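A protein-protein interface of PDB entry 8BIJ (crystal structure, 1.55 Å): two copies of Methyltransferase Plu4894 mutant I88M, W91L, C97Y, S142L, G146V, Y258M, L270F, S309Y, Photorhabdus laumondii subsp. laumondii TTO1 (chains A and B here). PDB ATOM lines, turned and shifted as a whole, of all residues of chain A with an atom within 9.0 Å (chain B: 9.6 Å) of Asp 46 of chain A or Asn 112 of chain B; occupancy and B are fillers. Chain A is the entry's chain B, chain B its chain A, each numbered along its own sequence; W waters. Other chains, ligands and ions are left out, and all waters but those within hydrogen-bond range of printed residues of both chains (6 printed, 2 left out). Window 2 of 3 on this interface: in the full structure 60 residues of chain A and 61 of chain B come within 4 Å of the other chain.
Among the printed residues, pairs that only touch across the chains: Arg 52 of chain A with Lys 282 of chain B (3.4 Å), Cys 43 of chain A with Leu 110 of chain B (3.5 Å), Arg 52 of chain A with Asp 276 of chain B (3.6 Å), Ile 45 of chain A with Leu 109 of chain B (3.6 Å), Arg 49 of chain A with Leu 109 of chain B (3.7 Å), Ile 45 of chain A with Asn 112 of chain B (3.7 Å), Leu 53 of chain A with Tyr 105 of chain B (3.7 Å), Ile 45 of chain A with Leu 110 of chain B (3.8 Å), Gly 44 of chain A with Leu 110 of chain B (3.8 Å), Leu 53 of chain A with Leu 109 of chain B (3.9 Å) and Gly 44 of chain A with Leu 109 of chain B (3.9 Å).
Water W4 bridges the backbone carbonyl oxygen of Leu 110 of chain B (2.6 Å) and the backbone carbonyl oxygen of Gly 44 of chain A (2.7 Å).
Water W1 lies within hydrogen-bond range of OG of Ser 280 of chain B (2.6 Å), OD1 of Asp 276 of chain B (2.9 Å) and NH1 of Arg 49 of chain A (3.3 Å).
Water W3 lies within hydrogen-bond range of the side-chain carboxylate (OD1) of Asp 276 of chain B (2.7 Å), the side-chain hydroxyl (OG) of Ser 108 of chain B (2.9 Å) and the guanidinium group (NH1) of Arg 49 of chain A (3.4 Å).
The side-chain amide nitrogen (ND2) of Asn 112 of chain B sits at hydrogen-bond distance from the backbone carbonyl oxygen (O) of Gly 44 of chain A (2.8 Å).
O of Ser 108 of chain B sits at hydrogen-bond distance from NH2 of Arg 49 of chain A (2.9 Å).
O of Gly 281 of chain B is in hydrogen-bond range of NH1 of Arg 52 of chain A (2.9 Å).
The side-chain carboxylate of Asp 276 of chain B is in salt-bridge range of the guanidinium group of Arg 49 of chain A (2.9 Å).
The side-chain amide oxygen of Asn 112 of chain B sits at hydrogen-bond distance from the backbone NH of Asp 46 of chain A (3.3 Å).
No position is printed for both chains.
Leu 39 of chain A touches none of the printed residues of chain B.
Of chain B, only Asn 112 (3.3 Å) comes within 4 Å of Asp 46 of chain A.
Asp 51 of chain A touches none of the printed residues of chain B.
Of the printed residues of chain B, Arg 52 of chain A touches Asp 276 (3.6 Å), Gly 281 (2.9 Å) and Lys 282 (3.4 Å).
Of the printed residues of chain A, Ser 108 of chain B touches Arg 49 (2.9 Å).
Of the printed residues of chain A, Leu 109 of chain B touches Gly 44, Ile 45, Arg 49 and Leu 53.
The nearest residue of chain B that does not touch Asp 46 of chain A is Leu 109 of chain B (4.4 Å).
The nearest residue of chain A that does not touch Asn 112 of chain B is Arg 49 of chain A (4.9 Å).
The backbone NH of Ile 45 of chain A lies within hydrogen-bond range of the backbone carbonyl oxygen of Ser 40 of chain A (3.1 Å).
The backbone carbonyl oxygen (O) of Leu 109 of chain B sits at hydrogen-bond distance from the side-chain amide nitrogen (ND2) of Asn 112 of chain B (3.0 Å).
OG of Ser 108 of chain B lies within hydrogen-bond range of O of Tyr 105 of chain B (2.7 Å).
SG of Cys 43 of chain A sits close to O of Leu 39 of chain A, 3.7 Å away.
Of the 19 printed residues of chain B, 8 touch a printed residue of chain A.
Printed residues of chain B that touch a printed residue of chain A: Tyr 105, Ser 108, Leu 109, Leu 110, Asn 112, Asp 276, Gly 281 and Lys 282.
Hydrophobic or aromatic side chains of chain B that line the printed part of chain A: Tyr 105, Leu 109 and Leu 110.
Of the 18 printed residues of chain A, 7 touch a printed residue of chain B.
Hydrophobic or aromatic side chains of chain A within 4 Å of the printed part of chain B: Ile 45 and Leu 53.
Along chain A the printed residues that touch a printed residue of chain B span positions 43 to 53.
Among the printed residues, 16 pairs touch across the chains.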
ATOM      1  N   LEU A  24     -19.893  31.570   2.627  1.00  0.00           N
ATOM      2  CA  LEU A  24     -19.228  31.128   1.372  1.00  0.00           C
ATOM      3  C   LEU A  24     -19.940  31.726   0.154  1.00  0.00           C
ATOM      4  O   LEU A  24     -19.236  32.150  -0.783  1.00  0.00           O
ATOM      5  CB  LEU A  24     -19.222  29.602   1.300  1.00  0.00           C
ATOM      6  CG  LEU A  24     -18.314  28.900   2.308  1.00  0.00           C
ATOM      7  CD1 LEU A  24     -18.659  27.426   2.376  1.00  0.00           C
ATOM      8  CD2 LEU A  24     -16.844  29.102   1.961  1.00  0.00           C
ATOM      9  N   ILE A  36     -10.690  27.561  -4.334  1.00  0.00           N
ATOM     10  CA  ILE A  36     -11.116  26.934  -3.046  1.00  0.00           C
ATOM     11  C   ILE A  36     -10.042  27.212  -1.986  1.00  0.00           C
ATOM     12  O   ILE A  36     -10.408  27.488  -0.828  1.00  0.00           O
ATOM     13  CB  ILE A  36     -11.412  25.432  -3.230  1.00  0.00           C
ATOM     14  CG1 ILE A  36     -12.611  25.215  -4.156  1.00  0.00           C
ATOM     15  CG2 ILE A  36     -11.614  24.751  -1.885  1.00  0.00           C
ATOM     16  CD1 ILE A  36     -12.782  23.792  -4.633  1.00  0.00           C
ATOM     17  N   ASP A  37      -8.768  27.178  -2.374  1.00  0.00           N
ATOM     18  CA  ASP A  37      -7.630  27.522  -1.480  1.00  0.00           C
ATOM     19  C   ASP A  37      -7.862  28.935  -0.921  1.00  0.00           C
ATOM     20  O   ASP A  37      -7.953  29.086   0.313  1.00  0.00           O
ATOM     21  CB  ASP A  37      -6.304  27.377  -2.231  1.00  0.00           C
ATOM     22  CG  ASP A  37      -5.067  27.466  -1.365  1.00  0.00           C
ATOM     23  OD1 ASP A  37      -5.191  27.847  -0.186  1.00  0.00           O
ATOM     24  OD2 ASP A  37      -3.984  27.133  -1.886  1.00  0.00           O
ATOM     25  N   LEU A  39     -10.561  30.742  -0.987  1.00  0.00           N
ATOM     26  CA  LEU A  39     -11.886  30.792  -0.307  1.00  0.00           C
ATOM     27  C   LEU A  39     -11.721  30.277   1.130  1.00  0.00           C
ATOM     28  O   LEU A  39     -12.218  30.927   2.058  1.00  0.00           O
ATOM     29  CB  LEU A  39     -12.900  29.971  -1.110  1.00  0.00           C
ATOM     30  CG  LEU A  39     -14.330  29.952  -0.572  1.00  0.00           C
ATOM     31  CD1 LEU A  39     -14.952  31.345  -0.598  1.00  0.00           C
ATOM     32  CD2 LEU A  39     -15.184  28.981  -1.372  1.00  0.00           C
ATOM     33  N   SER A  40     -10.995  29.172   1.316  1.00  0.00           N
ATOM     34  CA  SER A  40     -10.718  28.582   2.653  1.00  0.00           C
ATOM     35  C   SER A  40     -10.050  29.636   3.549  1.00  0.00           C
ATOM     36  O   SER A  40     -10.447  29.757   4.728  1.00  0.00           O
ATOM     37  CB  SER A  40      -9.913  27.294   2.547  1.00  0.00           C
ATOM     38  OG  SER A  40      -8.517  27.531   2.405  1.00  0.00           O
ATOM     39  N   ARG A  41      -9.103  30.401   2.998  1.00  0.00           N
ATOM     40  CA  ARG A  41      -8.309  31.409   3.753  1.00  0.00           C
ATOM     41  C   ARG A  41      -9.204  32.602   4.102  1.00  0.00           C
ATOM     42  O   ARG A  41      -9.121  33.090   5.241  1.00  0.00           O
ATOM     43  CB  ARG A  41      -7.079  31.834   2.946  1.00  0.00           C
ATOM     44  CG  ARG A  41      -6.103  30.696   2.682  1.00  0.00           C
ATOM     45  CD  ARG A  41      -5.058  31.029   1.631  1.00  0.00           C
ATOM     46  NE  ARG A  41      -4.204  29.882   1.371  1.00  0.00           N
ATOM     47  CZ  ARG A  41      -3.223  29.466   2.170  1.00  0.00           C
ATOM     48  NH1 ARG A  41      -2.951  30.109   3.293  1.00  0.00           N
ATOM     49  NH2 ARG A  41      -2.513  28.399   1.845  1.00  0.00           N
ATOM     50  N   CYS A  43     -12.561  32.690   4.451  1.00  0.00           N
ATOM     51  CA  CYS A  43     -13.731  32.335   5.303  1.00  0.00           C
ATOM     52  C   CYS A  43     -13.282  31.634   6.595  1.00  0.00           C
ATOM     53  O   CYS A  43     -14.138  31.439   7.482  1.00  0.00           O
ATOM     54  CB  CYS A  43     -14.728  31.484   4.521  1.00  0.00           C
ATOM     55  SG  CYS A  43     -15.489  32.367   3.131  1.00  0.00           S
ATOM     56  N   GLY A  44     -11.994  31.293   6.716  1.00  0.00           N
ATOM     57  CA  GLY A  44     -11.421  30.647   7.915  1.00  0.00           C
ATOM     58  C   GLY A  44     -11.955  29.235   8.103  1.00  0.00           C
ATOM     59  O   GLY A  44     -12.291  28.872   9.248  1.00  0.00           O
ATOM     60  N   ILE A  45     -12.045  28.470   7.012  1.00  0.00           N
ATOM     61  CA  ILE A  45     -12.512  27.054   7.014  1.00  0.00           C
ATOM     62  C   ILE A  45     -11.342  26.179   6.561  1.00  0.00           C
ATOM     63  O   ILE A  45     -10.639  26.554   5.606  1.00  0.00           O
ATOM     64  CB  ILE A  45     -13.757  26.862   6.125  1.00  0.00           C
ATOM     65  CG1 ILE A  45     -14.910  27.766   6.569  1.00  0.00           C
ATOM     66  CG2 ILE A  45     -14.181  25.402   6.090  1.00  0.00           C
ATOM     67  CD1 ILE A  45     -16.080  27.793   5.608  1.00  0.00           C
ATOM     68  N   ASP A  46     -11.141  25.055   7.238  1.00  0.00           N
ATOM     69  CA  ASP A  46     -10.114  24.057   6.854  1.00  0.00           C
ATOM     70  C   ASP A  46     -10.248  23.765   5.354  1.00  0.00           C
ATOM     71  O   ASP A  46     -11.373  23.422   4.910  1.00  0.00           O
ATOM     72  CB  ASP A  46     -10.267  22.791   7.691  1.00  0.00           C
ATOM     73  CG  ASP A  46      -9.301  21.700   7.276  1.00  0.00           C
ATOM     74  OD1 ASP A  46      -8.095  21.842   7.579  1.00  0.00           O
ATOM     75  OD2 ASP A  46      -9.757  20.737   6.621  1.00  0.00           O
ATOM     76  N   TYR A  47      -9.139  23.874   4.610  1.00  0.00           N
ATOM     77  CA  TYR A  47      -9.098  23.648   3.142  1.00  0.00           C
ATOM     78  C   TYR A  47      -9.744  22.301   2.783  1.00  0.00           C
ATOM     79  O   TYR A  47     -10.608  22.267   1.896  1.00  0.00           O
ATOM     80  CB  TYR A  47      -7.674  23.693   2.583  1.00  0.00           C
ATOM     81  CG  TYR A  47      -7.625  23.281   1.134  1.00  0.00           C
ATOM     82  CD1 TYR A  47      -7.937  24.173   0.125  1.00  0.00           C
ATOM     83  CD2 TYR A  47      -7.350  21.973   0.771  1.00  0.00           C
ATOM     84  CE1 TYR A  47      -7.932  23.791  -1.208  1.00  0.00           C
ATOM     85  CE2 TYR A  47      -7.354  21.573  -0.555  1.00  0.00           C
ATOM     86  CZ  TYR A  47      -7.642  22.486  -1.553  1.00  0.00           C
ATOM     87  OH  TYR A  47      -7.639  22.093  -2.861  1.00  0.00           O
ATOM     88  N   SER A  48      -9.292  21.198   3.388  1.00  0.00           N
ATOM     89  CA  SER A  48      -9.778  19.838   3.042  1.00  0.00           C
ATOM     90  C   SER A  48     -11.289  19.729   3.286  1.00  0.00           C
ATOM     91  O   SER A  48     -12.002  19.189   2.419  1.00  0.00           O
ATOM     92  CB  SER A  48      -9.023  18.774   3.803  1.00  0.00           C
ATOM     93  OG  SER A  48      -9.517  17.483   3.481  1.00  0.00           O
ATOM     94  N   ARG A  49     -11.772  20.227   4.426  1.00  0.00           N
ATOM     95  CA  ARG A  49     -13.212  20.147   4.775  1.00  0.00           C
ATOM     96  C   ARG A  49     -14.015  21.013   3.794  1.00  0.00           C
ATOM     97  O   ARG A  49     -15.090  20.565   3.373  1.00  0.00           O
ATOM     98  CB  ARG A  49     -13.435  20.580   6.222  1.00  0.00           C
ATOM     99  CG  ARG A  49     -12.903  19.594   7.247  1.00  0.00           C
ATOM    100  CD  ARG A  49     -13.209  20.095   8.636  1.00  0.00           C
ATOM    101  NE  ARG A  49     -14.636  20.037   8.907  1.00  0.00           N
ATOM    102  CZ  ARG A  49     -15.263  20.760   9.832  1.00  0.00           C
ATOM    103  NH1 ARG A  49     -16.567  20.615  10.005  1.00  0.00           N
ATOM    104  NH2 ARG A  49     -14.585  21.600  10.595  1.00  0.00           N
ATOM    105  N   LEU A  50     -13.486  22.173   3.400  1.00  0.00           N
ATOM    106  CA  LEU A  50     -14.186  23.065   2.429  1.00  0.00           C
ATOM    107  C   LEU A  50     -14.185  22.380   1.059  1.00  0.00           C
ATOM    108  O   LEU A  50     -15.224  22.376   0.389  1.00  0.00           O
ATOM    109  CB  LEU A  50     -13.512  24.439   2.366  1.00  0.00           C
ATOM    110  CG  LEU A  50     -14.089  25.401   1.319  1.00  0.00           C
ATOM    111  CD1 LEU A  50     -15.580  25.648   1.529  1.00  0.00           C
ATOM    112  CD2 LEU A  50     -13.333  26.718   1.319  1.00  0.00           C
ATOM    113  N   ASP A  51     -13.060  21.780   0.663  1.00  0.00           N
ATOM    114  CA  ASP A  51     -12.958  21.086  -0.647  1.00  0.00           C
ATOM    115  C   ASP A  51     -13.986  19.944  -0.702  1.00  0.00           C
ATOM    116  O   ASP A  51     -14.599  19.728  -1.789  1.00  0.00           O
ATOM    117  CB  ASP A  51     -11.544  20.550  -0.896  1.00  0.00           C
ATOM    118  CG  ASP A  51     -11.282  20.172  -2.343  1.00  0.00           C
ATOM    119  OD1 ASP A  51     -11.916  20.766  -3.238  1.00  0.00           O
ATOM    120  OD2 ASP A  51     -10.440  19.297  -2.564  1.00  0.00           O
ATOM    121  N   ARG A  52     -14.154  19.213   0.411  1.00  0.00           N
ATOM    122  CA  ARG A  52     -15.121  18.088   0.500  1.00  0.00           C
ATOM    123  C   ARG A  52     -16.553  18.629   0.389  1.00  0.00           C
ATOM    124  O   ARG A  52     -17.356  18.019  -0.333  1.00  0.00           O
ATOM    125  CB  ARG A  52     -14.877  17.279   1.777  1.00  0.00           C
ATOM    126  CG  ARG A  52     -13.607  16.444   1.711  1.00  0.00           C
ATOM    127  CD  ARG A  52     -13.120  16.044   3.089  1.00  0.00           C
ATOM    128  NE  ARG A  52     -14.146  15.290   3.798  1.00  0.00           N
ATOM    129  CZ  ARG A  52     -14.231  15.152   5.117  1.00  0.00           C
ATOM    130  NH1 ARG A  52     -15.222  14.442   5.636  1.00  0.00           N
ATOM    131  NH2 ARG A  52     -13.344  15.725   5.914  1.00  0.00           N
ATOM    132  N   LEU A  53     -16.852  19.732   1.075  1.00  0.00           N
ATOM    133  CA  LEU A  53     -18.188  20.385   0.975  1.00  0.00           C
ATOM    134  C   LEU A  53     -18.430  20.816  -0.475  1.00  0.00           C
ATOM    135  O   LEU A  53     -19.525  20.545  -0.981  1.00  0.00           O
ATOM    136  CB  LEU A  53     -18.268  21.569   1.939  1.00  0.00           C
ATOM    137  CG  LEU A  53     -19.509  22.459   1.788  1.00  0.00           C
ATOM    138  CD1 LEU A  53     -20.784  21.649   1.947  1.00  0.00           C
ATOM    139  CD2 LEU A  53     -19.462  23.572   2.810  1.00  0.00           C
ATOM    140  N   CYS A  54     -17.434  21.432  -1.120  1.00  0.00           N
ATOM    141  CA  CYS A  54     -17.512  21.855  -2.543  1.00  0.00           C
ATOM    142  C   CYS A  54     -17.722  20.621  -3.435  1.00  0.00           C
ATOM    143  O   CYS A  54     -18.556  20.684  -4.343  1.00  0.00           O
ATOM    144  CB  CYS A  54     -16.303  22.688  -2.953  1.00  0.00           C
ATOM    145  SG  CYS A  54     -16.323  24.359  -2.250  1.00  0.00           S
ATOM    146  N   MET B 104     -25.340  22.112  13.704  1.00  0.00           N
ATOM    147  CA  MET B 104     -24.017  22.608  14.172  1.00  0.00           C
ATOM    148  C   MET B 104     -22.931  22.413  13.103  1.00  0.00           C
ATOM    149  O   MET B 104     -21.775  22.758  13.394  1.00  0.00           O
ATOM    150  CB  MET B 104     -23.606  21.919  15.475  1.00  0.00           C
ATOM    151  CG  MET B 104     -24.440  22.354  16.670  1.00  0.00           C
ATOM    152  SD  MET B 104     -24.299  24.133  17.037  1.00  0.00           S
ATOM    153  CE  MET B 104     -25.896  24.741  16.504  1.00  0.00           C
ATOM    154  N   TYR B 105     -23.286  21.979  11.889  1.00  0.00           N
ATOM    155  CA  TYR B 105     -22.316  21.792  10.775  1.00  0.00           C
ATOM    156  C   TYR B 105     -21.701  23.140  10.388  1.00  0.00           C
ATOM    157  O   TYR B 105     -20.487  23.273  10.302  1.00  0.00           O
ATOM    158  CB  TYR B 105     -22.955  21.018   9.620  1.00  0.00           C
ATOM    159  CG  TYR B 105     -22.054  20.799   8.431  1.00  0.00           C
ATOM    160  CD1 TYR B 105     -20.803  20.213   8.573  1.00  0.00           C
ATOM    161  CD2 TYR B 105     -22.473  21.101   7.149  1.00  0.00           C
ATOM    162  CE1 TYR B 105     -19.977  20.001   7.479  1.00  0.00           C
ATOM    163  CE2 TYR B 105     -21.664  20.896   6.044  1.00  0.00           C
ATOM    164  CZ  TYR B 105     -20.411  20.332   6.205  1.00  0.00           C
ATOM    165  OH  TYR B 105     -19.622  20.121   5.106  1.00  0.00           O
ATOM    166  N   PRO B 106     -22.479  24.228  10.166  1.00  0.00           N
ATOM    167  CA  PRO B 106     -21.850  25.509   9.848  1.00  0.00           C
ATOM    168  C   PRO B 106     -20.861  25.981  10.932  1.00  0.00           C
ATOM    169  O   PRO B 106     -19.754  26.399  10.595  1.00  0.00           O
ATOM    170  CB  PRO B 106     -23.050  26.467   9.708  1.00  0.00           C
ATOM    171  CG  PRO B 106     -24.210  25.559   9.373  1.00  0.00           C
ATOM    172  CD  PRO B 106     -23.949  24.295  10.168  1.00  0.00           C
ATOM    173  N   ARG B 107     -21.281  25.932  12.203  1.00  0.00           N
ATOM    174  CA  ARG B 107     -20.417  26.308  13.353  1.00  0.00           C
ATOM    175  C   ARG B 107     -19.140  25.450  13.338  1.00  0.00           C
ATOM    176  O   ARG B 107     -18.043  25.993  13.550  1.00  0.00           O
ATOM    177  CB  ARG B 107     -21.156  26.121  14.678  1.00  0.00           C
ATOM    178  CG  ARG B 107     -20.360  26.596  15.881  1.00  0.00           C
ATOM    179  CD  ARG B 107     -21.192  26.623  17.144  1.00  0.00           C
ATOM    180  NE  ARG B 107     -20.335  26.499  18.309  1.00  0.00           N
ATOM    181  CZ  ARG B 107     -20.751  26.198  19.531  1.00  0.00           C
ATOM    182  NH1 ARG B 107     -19.869  26.081  20.511  1.00  0.00           N
ATOM    183  NH2 ARG B 107     -22.038  26.011  19.768  1.00  0.00           N
ATOM    184  N   SER B 108     -19.277  24.148  13.084  1.00  0.00           N
ATOM    185  CA  SER B 108     -18.138  23.193  13.058  1.00  0.00           C
ATOM    186  C   SER B 108     -17.134  23.601  11.971  1.00  0.00           C
ATOM    187  O   SER B 108     -15.923  23.521  12.236  1.00  0.00           O
ATOM    188  CB  SER B 108     -18.618  21.775  12.885  1.00  0.00           C
ATOM    189  OG  SER B 108     -18.940  21.495  11.531  1.00  0.00           O
ATOM    190  N   LEU B 109     -17.617  24.031  10.800  1.00  0.00           N
ATOM    191  CA  LEU B 109     -16.762  24.495   9.672  1.00  0.00           C
ATOM    192  C   LEU B 109     -15.952  25.737  10.065  1.00  0.00           C
ATOM    193  O   LEU B 109     -14.790  25.843   9.627  1.00  0.00           O
ATOM    194  CB  LEU B 109     -17.641  24.778   8.449  1.00  0.00           C
ATOM    195  CG  LEU B 109     -18.158  23.534   7.728  1.00  0.00           C
ATOM    196  CD1 LEU B 109     -19.229  23.891   6.717  1.00  0.00           C
ATOM    197  CD2 LEU B 109     -17.029  22.784   7.044  1.00  0.00           C
ATOM    198  N   LEU B 110     -16.540  26.660  10.830  1.00  0.00           N
ATOM    199  CA  LEU B 110     -15.898  27.957  11.172  1.00  0.00           C
ATOM    200  C   LEU B 110     -15.002  27.841  12.414  1.00  0.00           C
ATOM    201  O   LEU B 110     -14.175  28.747  12.600  1.00  0.00           O
ATOM    202  CB  LEU B 110     -16.983  29.018  11.364  1.00  0.00           C
ATOM    203  CG  LEU B 110     -17.778  29.348  10.104  1.00  0.00           C
ATOM    204  CD1 LEU B 110     -18.911  30.310  10.423  1.00  0.00           C
ATOM    205  CD2 LEU B 110     -16.872  29.921   9.026  1.00  0.00           C
ATOM    206  N   GLU B 111     -15.117  26.779  13.213  1.00  0.00           N
ATOM    207  CA  GLU B 111     -14.388  26.671  14.512  1.00  0.00           C
ATOM    208  C   GLU B 111     -12.961  26.127  14.327  1.00  0.00           C
ATOM    209  O   GLU B 111     -12.086  26.564  15.098  1.00  0.00           O
ATOM    210  CB  GLU B 111     -15.225  25.885  15.522  1.00  0.00           C
ATOM    211  CG  GLU B 111     -16.400  26.710  16.027  1.00  0.00           C
ATOM    212  CD  GLU B 111     -16.923  26.387  17.414  1.00  0.00           C
ATOM    213  OE1 GLU B 111     -17.603  27.264  17.998  1.00  0.00           O
ATOM    214  OE2 GLU B 111     -16.666  25.264  17.902  1.00  0.00           O
ATOM    215  N   ASN B 112     -12.713  25.227  13.370  1.00  0.00           N
ATOM    216  CA  ASN B 112     -11.343  24.740  13.024  1.00  0.00           C
ATOM    217  C   ASN B 112     -10.584  24.194  14.247  1.00  0.00           C
ATOM    218  O   ASN B 112      -9.341  24.331  14.266  1.00  0.00           O
ATOM    219  CB  ASN B 112     -10.471  25.846  12.421  1.00  0.00           C
ATOM    220  CG  ASN B 112     -10.732  26.087  10.951  1.00  0.00           C
ATOM    221  OD1 ASN B 112      -9.814  25.989  10.140  1.00  0.00           O
ATOM    222  ND2 ASN B 112     -11.970  26.403  10.606  1.00  0.00           N
ATOM    223  N   ASP B 113     -11.269  23.588  15.221  1.00  0.00           N
ATOM    224  CA  ASP B 113     -10.623  22.915  16.385  1.00  0.00           C
ATOM    225  C   ASP B 113     -10.692  21.396  16.180  1.00  0.00           C
ATOM    226  O   ASP B 113     -10.294  20.654  17.098  1.00  0.00           O
ATOM    227  CB  ASP B 113     -11.262  23.336  17.712  1.00  0.00           C
ATOM    228  CG  ASP B 113     -12.779  23.248  17.726  1.00  0.00           C
ATOM    229  OD1 ASP B 113     -13.337  22.658  16.783  1.00  0.00           O
ATOM    230  OD2 ASP B 113     -13.391  23.791  18.670  1.00  0.00           O
ATOM    231  N   GLY B 114     -11.202  20.957  15.024  1.00  0.00           N
ATOM    232  CA  GLY B 114     -11.357  19.537  14.665  1.00  0.00           C
ATOM    233  C   GLY B 114     -12.559  18.866  15.317  1.00  0.00           C
ATOM    234  O   GLY B 114     -12.717  17.655  15.125  1.00  0.00           O
ATOM    235  N   LYS B 115     -13.386  19.617  16.052  1.00  0.00           N
ATOM    236  CA  LYS B 115     -14.579  19.070  16.750  1.00  0.00           C
ATOM    237  C   LYS B 115     -15.735  18.974  15.759  1.00  0.00           C
ATOM    238  O   LYS B 115     -16.125  19.972  15.153  1.00  0.00           O
ATOM    239  CB  LYS B 115     -14.942  19.918  17.971  1.00  0.00           C
ATOM    240  CG  LYS B 115     -14.243  19.485  19.252  1.00  0.00           C
ATOM    241  CD  LYS B 115     -14.410  20.451  20.396  1.00  0.00           C
ATOM    242  CE  LYS B 115     -15.834  20.523  20.904  1.00  0.00           C
ATOM    243  NZ  LYS B 115     -16.079  21.784  21.639  1.00  0.00           N
ATOM    244  N   PRO B 116     -16.314  17.766  15.567  1.00  0.00           N
ATOM    245  CA  PRO B 116     -17.413  17.582  14.625  1.00  0.00           C
ATOM    246  C   PRO B 116     -18.713  18.214  15.152  1.00  0.00           C
ATOM    247  O   PRO B 116     -18.847  18.403  16.354  1.00  0.00           O
ATOM    248  CB  PRO B 116     -17.528  16.056  14.502  1.00  0.00           C
ATOM    249  CG  PRO B 116     -16.980  15.520  15.809  1.00  0.00           C
ATOM    250  CD  PRO B 116     -15.940  16.522  16.263  1.00  0.00           C
ATOM    251  N   ILE B 120     -20.123  19.128  19.102  1.00  0.00           N
ATOM    252  CA  ILE B 120     -20.587  20.487  19.495  1.00  0.00           C
ATOM    253  C   ILE B 120     -22.018  20.347  20.035  1.00  0.00           C
ATOM    254  O   ILE B 120     -22.309  20.949  21.081  1.00  0.00           O
ATOM    255  CB  ILE B 120     -20.467  21.467  18.316  1.00  0.00           C
ATOM    256  CG1 ILE B 120     -19.013  21.642  17.865  1.00  0.00           C
ATOM    257  CG2 ILE B 120     -21.097  22.798  18.679  1.00  0.00           C
ATOM    258  CD1 ILE B 120     -18.850  22.432  16.585  1.00  0.00           C
ATOM    259  N   ASP B 234      -6.708  11.710   9.404  1.00  0.00           N
ATOM    260  CA  ASP B 234      -5.493  11.092   8.812  1.00  0.00           C
ATOM    261  C   ASP B 234      -4.557  10.638   9.941  1.00  0.00           C
ATOM    262  O   ASP B 234      -4.068   9.494   9.880  1.00  0.00           O
ATOM    263  CB  ASP B 234      -4.794  12.053   7.852  1.00  0.00           C
ATOM    264  CG  ASP B 234      -5.495  12.198   6.511  1.00  0.00           C
ATOM    265  OD1 ASP B 234      -6.568  11.582   6.330  1.00  0.00           O
ATOM    266  OD2 ASP B 234      -4.955  12.921   5.654  1.00  0.00           O
ATOM    267  N   ASP B 276     -17.968  13.731   8.339  1.00  0.00           N
ATOM    268  CA  ASP B 276     -17.494  15.038   8.873  1.00  0.00           C
ATOM    269  C   ASP B 276     -18.374  15.422  10.069  1.00  0.00           C
ATOM    270  O   ASP B 276     -17.818  15.700  11.156  1.00  0.00           O
ATOM    271  CB  ASP B 276     -17.517  16.139   7.807  1.00  0.00           C
ATOM    272  CG  ASP B 276     -17.009  17.487   8.294  1.00  0.00           C
ATOM    273  OD1 ASP B 276     -17.351  17.871   9.431  1.00  0.00           O
ATOM    274  OD2 ASP B 276     -16.271  18.147   7.534  1.00  0.00           O
ATOM    275  N   SER B 280     -15.677  13.911  12.416  1.00  0.00           N
ATOM    276  CA  SER B 280     -14.522  14.563  11.750  1.00  0.00           C
ATOM    277  C   SER B 280     -13.722  13.463  11.042  1.00  0.00           C
ATOM    278  O   SER B 280     -12.481  13.549  11.003  1.00  0.00           O
ATOM    279  CB  SER B 280     -13.678  15.357  12.726  1.00  0.00           C
ATOM    280  OG  SER B 280     -14.437  16.391  13.343  1.00  0.00           O
ATOM    281  N   GLY B 281     -14.440  12.460  10.525  1.00  0.00           N
ATOM    282  CA  GLY B 281     -13.898  11.407   9.648  1.00  0.00           C
ATOM    283  C   GLY B 281     -14.025  11.832   8.199  1.00  0.00           C
ATOM    284  O   GLY B 281     -14.345  13.009   7.941  1.00  0.00           O
ATOM    285  N   LYS B 282     -13.786  10.911   7.267  1.00  0.00           N
ATOM    286  CA  LYS B 282     -13.867  11.175   5.808  1.00  0.00           C
ATOM    287  C   LYS B 282     -13.824   9.850   5.048  1.00  0.00           C
ATOM    288  O   LYS B 282     -13.301   8.859   5.606  1.00  0.00           O
ATOM    289  CB  LYS B 282     -12.726  12.090   5.350  1.00  0.00           C
ATOM    290  CG  LYS B 282     -11.326  11.508   5.481  1.00  0.00           C
ATOM    291  CD  LYS B 282     -10.239  12.411   4.930  1.00  0.00           C
ATOM    292  CE  LYS B 282     -10.426  12.741   3.464  1.00  0.00           C
ATOM    293  NZ  LYS B 282      -9.196  13.317   2.870  1.00  0.00           N
HETATM  294  O   HOH W   1     -15.298  18.030  11.512  1.00  0.00           O
HETATM  295  O   HOH W   2      -7.219  23.842   9.409  1.00  0.00           O
HETATM  296  O   HOH W   3     -18.825  18.601  11.563  1.00  0.00           O
HETATM  297  O   HOH W   4     -13.534  30.597  10.902  1.00  0.00           O
HETATM  298  O   HOH W   5     -17.099  19.167   5.215  1.00  0.00           O
HETATM  299  O   HOH W   6     -13.642  15.654   8.763  1.00  0.00           O
